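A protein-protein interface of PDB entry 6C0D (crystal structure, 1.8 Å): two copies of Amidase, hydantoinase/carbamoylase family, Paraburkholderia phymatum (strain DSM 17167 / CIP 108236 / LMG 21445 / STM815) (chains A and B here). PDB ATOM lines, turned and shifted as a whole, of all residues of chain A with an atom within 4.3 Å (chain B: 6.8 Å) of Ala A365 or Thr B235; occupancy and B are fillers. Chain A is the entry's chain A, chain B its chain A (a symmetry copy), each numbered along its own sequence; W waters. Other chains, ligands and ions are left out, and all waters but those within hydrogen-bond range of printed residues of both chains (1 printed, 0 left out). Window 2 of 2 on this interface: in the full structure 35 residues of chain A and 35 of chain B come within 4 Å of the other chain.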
ATOM      1  N   GLY A 200      23.767  10.000 -10.373  1.00  0.00           N
ATOM      2  CA  GLY A 200      23.420  10.489  -9.043  1.00  0.00           C
ATOM      3  C   GLY A 200      23.235   9.396  -8.009  1.00  0.00           C
ATOM      4  O   GLY A 200      23.689   9.527  -6.866  1.00  0.00           O
ATOM      5  N   ILE A 216      10.563  15.832 -14.425  1.00  0.00           N
ATOM      6  CA  ILE A 216      11.785  16.574 -14.123  1.00  0.00           C
ATOM      7  C   ILE A 216      11.480  17.532 -12.971  1.00  0.00           C
ATOM      8  O   ILE A 216      10.538  18.328 -13.054  1.00  0.00           O
ATOM      9  CB  ILE A 216      12.285  17.317 -15.369  1.00  0.00           C
ATOM     10  CG1 ILE A 216      12.623  16.288 -16.464  1.00  0.00           C
ATOM     11  CG2 ILE A 216      13.491  18.197 -15.045  1.00  0.00           C
ATOM     12  CD1 ILE A 216      12.983  16.930 -17.807  1.00  0.00           C
ATOM     13  N   ARG A 295      14.370  20.650  -4.170  1.00  0.00           N
ATOM     14  CA  ARG A 295      13.782  20.161  -5.417  1.00  0.00           C
ATOM     15  C   ARG A 295      12.719  19.129  -5.106  1.00  0.00           C
ATOM     16  O   ARG A 295      12.846  18.363  -4.150  1.00  0.00           O
ATOM     17  CB  ARG A 295      14.822  19.507  -6.345  1.00  0.00           C
ATOM     18  CG  ARG A 295      16.090  20.338  -6.555  1.00  0.00           C
ATOM     19  CD  ARG A 295      16.970  19.739  -7.659  1.00  0.00           C
ATOM     20  NE  ARG A 295      18.316  20.318  -7.630  1.00  0.00           N
ATOM     21  CZ  ARG A 295      19.125  20.396  -8.681  1.00  0.00           C
ATOM     22  NH1 ARG A 295      18.725  19.938  -9.863  1.00  0.00           N
ATOM     23  NH2 ARG A 295      20.326  20.956  -8.560  1.00  0.00           N
ATOM     24  N   SER A 363      13.535  12.694 -12.574  1.00  0.00           N
ATOM     25  CA  SER A 363      14.857  13.229 -12.865  1.00  0.00           C
ATOM     26  C   SER A 363      15.171  14.345 -11.878  1.00  0.00           C
ATOM     27  O   SER A 363      14.516  15.394 -11.893  1.00  0.00           O
ATOM     28  CB  SER A 363      14.957  13.760 -14.295  1.00  0.00           C
ATOM     29  OG  SER A 363      16.190  14.460 -14.446  1.00  0.00           O
ATOM     30  N   GLY A 364      16.197  14.140 -11.044  1.00  0.00           N
ATOM     31  CA  GLY A 364      16.566  15.184 -10.105  1.00  0.00           C
ATOM     32  C   GLY A 364      17.366  16.318 -10.710  1.00  0.00           C
ATOM     33  O   GLY A 364      17.627  17.314 -10.027  1.00  0.00           O
ATOM     34  N   ALA A 365      17.761  16.185 -11.975  1.00  0.00           N
ATOM     35  CA  ALA A 365      18.558  17.187 -12.672  1.00  0.00           C
ATOM     36  C   ALA A 365      17.770  17.760 -13.845  1.00  0.00           C
ATOM     37  O   ALA A 365      16.834  17.136 -14.336  1.00  0.00           O
ATOM     38  CB  ALA A 365      19.869  16.584 -13.198  1.00  0.00           C
ATOM     39  N   SER A 366      18.191  18.931 -14.313  1.00  0.00           N
ATOM     40  CA  SER A 366      17.542  19.573 -15.447  1.00  0.00           C
ATOM     41  C   SER A 366      18.143  19.083 -16.765  1.00  0.00           C
ATOM     42  O   SER A 366      19.288  18.633 -16.825  1.00  0.00           O
ATOM     43  CB  SER A 366      17.654  21.097 -15.337  1.00  0.00           C
ATOM     44  OG  SER A 366      18.992  21.525 -15.199  1.00  0.00           O
ATOM     45  N   HIS A 367      17.348  19.179 -17.829  1.00  0.00           N
ATOM     46  CA  HIS A 367      17.707  18.665 -19.151  1.00  0.00           C
ATOM     47  C   HIS A 367      16.973  19.476 -20.206  1.00  0.00           C
ATOM     48  O   HIS A 367      15.974  20.128 -19.914  1.00  0.00           O
ATOM     49  CB  HIS A 367      17.321  17.190 -19.344  1.00  0.00           C
ATOM     50  CG  HIS A 367      17.903  16.276 -18.314  1.00  0.00           C
ATOM     51  ND1 HIS A 367      19.234  15.919 -18.316  1.00  0.00           N
ATOM     52  CD2 HIS A 367      17.345  15.659 -17.243  1.00  0.00           C
ATOM     53  CE1 HIS A 367      19.474  15.124 -17.286  1.00  0.00           C
ATOM     54  NE2 HIS A 367      18.344  14.943 -16.624  1.00  0.00           N
ATOM     55  N   ASN B 231      28.222  14.844  -3.598  1.00  0.00           N
ATOM     56  CA  ASN B 231      27.163  14.258  -4.419  1.00  0.00           C
ATOM     57  C   ASN B 231      26.392  15.376  -5.106  1.00  0.00           C
ATOM     58  O   ASN B 231      26.396  16.528  -4.668  1.00  0.00           O
ATOM     59  CB  ASN B 231      26.174  13.414  -3.598  1.00  0.00           C
ATOM     60  CG  ASN B 231      26.599  11.967  -3.419  1.00  0.00           C
ATOM     61  OD1 ASN B 231      26.776  11.507  -2.286  1.00  0.00           O
ATOM     62  ND2 ASN B 231      26.691  11.218  -4.527  1.00  0.00           N
ATOM     63  N   HIS B 232      25.726  15.014  -6.194  1.00  0.00           N
ATOM     64  CA  HIS B 232      24.853  15.950  -6.890  1.00  0.00           C
ATOM     65  C   HIS B 232      23.631  16.224  -6.015  1.00  0.00           C
ATOM     66  O   HIS B 232      22.942  15.286  -5.599  1.00  0.00           O
ATOM     67  CB  HIS B 232      24.464  15.339  -8.235  1.00  0.00           C
ATOM     68  CG  HIS B 232      23.700  16.263  -9.136  1.00  0.00           C
ATOM     69  ND1 HIS B 232      22.480  16.801  -8.789  1.00  0.00           N
ATOM     70  CD2 HIS B 232      23.963  16.706 -10.391  1.00  0.00           C
ATOM     71  CE1 HIS B 232      22.038  17.563  -9.777  1.00  0.00           C
ATOM     72  NE2 HIS B 232      22.920  17.526 -10.761  1.00  0.00           N
ATOM     73  N   ALA B 233      23.370  17.503  -5.718  1.00  0.00           N
ATOM     74  CA  ALA B 233      22.321  17.847  -4.760  1.00  0.00           C
ATOM     75  C   ALA B 233      20.910  17.611  -5.289  1.00  0.00           C
ATOM     76  O   ALA B 233      19.958  17.677  -4.500  1.00  0.00           O
ATOM     77  CB  ALA B 233      22.448  19.311  -4.337  1.00  0.00           C
ATOM     78  N   GLY B 234      20.748  17.392  -6.589  1.00  0.00           N
ATOM     79  CA  GLY B 234      19.434  17.145  -7.162  1.00  0.00           C
ATOM     80  C   GLY B 234      19.149  15.662  -7.332  1.00  0.00           C
ATOM     81  O   GLY B 234      18.045  15.189  -7.062  1.00  0.00           O
ATOM     82  N   THR B 235      20.147  14.899  -7.762  1.00  0.00           N
ATOM     83  CA  THR B 235      19.893  13.518  -8.126  1.00  0.00           C
ATOM     84  C   THR B 235      20.111  12.539  -6.979  1.00  0.00           C
ATOM     85  O   THR B 235      19.654  11.397  -7.073  1.00  0.00           O
ATOM     86  CB  THR B 235      20.786  13.120  -9.305  1.00  0.00           C
ATOM     87  OG1 THR B 235      22.147  13.269  -8.917  1.00  0.00           O
ATOM     88  CG2 THR B 235      20.554  14.045 -10.481  1.00  0.00           C
ATOM     89  N   THR B 236      20.792  12.956  -5.900  1.00  0.00           N
ATOM     90  CA  THR B 236      21.141  12.047  -4.808  1.00  0.00           C
ATOM     91  C   THR B 236      20.037  12.001  -3.756  1.00  0.00           C
ATOM     92  O   THR B 236      19.809  13.013  -3.074  1.00  0.00           O
ATOM     93  CB  THR B 236      22.450  12.473  -4.159  1.00  0.00           C
ATOM     94  OG1 THR B 236      23.459  12.555  -5.168  1.00  0.00           O
ATOM     95  CG2 THR B 236      22.877  11.423  -3.099  1.00  0.00           C
ATOM     96  N   PRO B 237      19.351  10.866  -3.567  1.00  0.00           N
ATOM     97  CA  PRO B 237      18.276  10.815  -2.568  1.00  0.00           C
ATOM     98  C   PRO B 237      18.821  11.110  -1.177  1.00  0.00           C
ATOM     99  O   PRO B 237      19.971  10.796  -0.866  1.00  0.00           O
ATOM    100  CB  PRO B 237      17.757   9.373  -2.667  1.00  0.00           C
ATOM    101  CG  PRO B 237      18.183   8.898  -4.043  1.00  0.00           C
ATOM    102  CD  PRO B 237      19.483   9.596  -4.314  1.00  0.00           C
ATOM    103  N   ILE B 240      20.688   8.317   1.092  1.00  0.00           N
ATOM    104  CA  ILE B 240      22.022   7.770   0.867  1.00  0.00           C
ATOM    105  C   ILE B 240      23.108   8.839   0.978  1.00  0.00           C
ATOM    106  O   ILE B 240      24.264   8.581   0.624  1.00  0.00           O
ATOM    107  CB  ILE B 240      22.108   7.020  -0.474  1.00  0.00           C
ATOM    108  CG1 ILE B 240      21.955   7.972  -1.658  1.00  0.00           C
ATOM    109  CG2 ILE B 240      21.047   5.905  -0.527  1.00  0.00           C
ATOM    110  CD1 ILE B 240      22.045   7.295  -3.019  1.00  0.00           C
ATOM    111  N   ARG B 241      22.784  10.009   1.524  1.00  0.00           N
ATOM    112  CA  ARG B 241      23.759  11.094   1.580  1.00  0.00           C
ATOM    113  C   ARG B 241      24.730  10.946   2.739  1.00  0.00           C
ATOM    114  O   ARG B 241      24.423  10.351   3.771  1.00  0.00           O
ATOM    115  CB  ARG B 241      23.054  12.445   1.705  1.00  0.00           C
ATOM    116  CG  ARG B 241      22.399  12.825   0.399  1.00  0.00           C
ATOM    117  CD  ARG B 241      21.724  14.177   0.496  1.00  0.00           C
ATOM    118  NE  ARG B 241      21.096  14.438  -0.801  1.00  0.00           N
ATOM    119  CZ  ARG B 241      20.761  15.639  -1.223  1.00  0.00           C
ATOM    120  NH1 ARG B 241      20.978  16.695  -0.433  1.00  0.00           N
ATOM    121  NH2 ARG B 241      20.184  15.769  -2.429  1.00  0.00           N
HETATM  122  O   HOH W   1      23.961  12.684 -11.025  1.00  0.00           O
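ND1 of His B232 is in hydrogen-bond range of N of Thr B235, at 3.2 Å. ND1 of His B232 is in hydrogen-bond range of N of Gly B234. NH1 of Arg A295 sits at hydrogen-bond distance from O of Gly A364 (2.8 Å). The backbone carbonyl oxygen (O) of His B232 lies within hydrogen-bond range of the side-chain hydroxyl (OG1) of Thr B236. NH2 of Arg B241 sits at hydrogen-bond distance from O of Thr B236. The side-chain hydroxyl of Ser A363 lies within hydrogen-bond range of the backbone carbonyl oxygen of Ala A365.
Of the 9 printed residues of chain B, 4 touch a printed residue of chain A. Printed residues of chain B that touch a printed residue of chain A: His B232, Gly B234, Thr B235 and Thr B236. Among the printed residues, no Asp or Glu carboxylate lies within 4 Å of a Lys or Arg side-chain nitrogen of the other chain.
Water W1 lies within hydrogen-bond range of the backbone NH of Gly A200 and the side-chain hydroxyl of Thr B235.
OG1 of Thr B236 is in hydrogen-bond range of O of Gly A200 (3.5 Å).
No position is printed for both chains. Of the 7 pairs that touch across the chains among the printed residues, none has its exchanged pair printed and touching as well.
Of the printed residues of chain B, Ala A365 touches Thr B235. Thr B235 touches just these residues of chain A: Gly A200 (3.1 Å), Gly A364 (3.9 Å) and Ala A365 (3.8 Å). Printed residues of chain A within 4 Å of Gly B234: Arg A295 and Gly A364. Of the printed residues of chain B, Gly A200 touches Thr B235 (3.1 Å) and Thr B236 (3.5 Å). Ala B233 touches none of the printed residues of chain A.
Gly A200 touches Thr B235. Arg A295 touches His B232 (NH2 to CE1, 3.99 Å). Gly B234 touches Arg A295. CA of Gly A364 touches O of Gly B234, 3.4 Å away. C of Gly A364 touches CG2 of Thr B235, at 3.9 Å. Ala A365 touches Thr B235.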
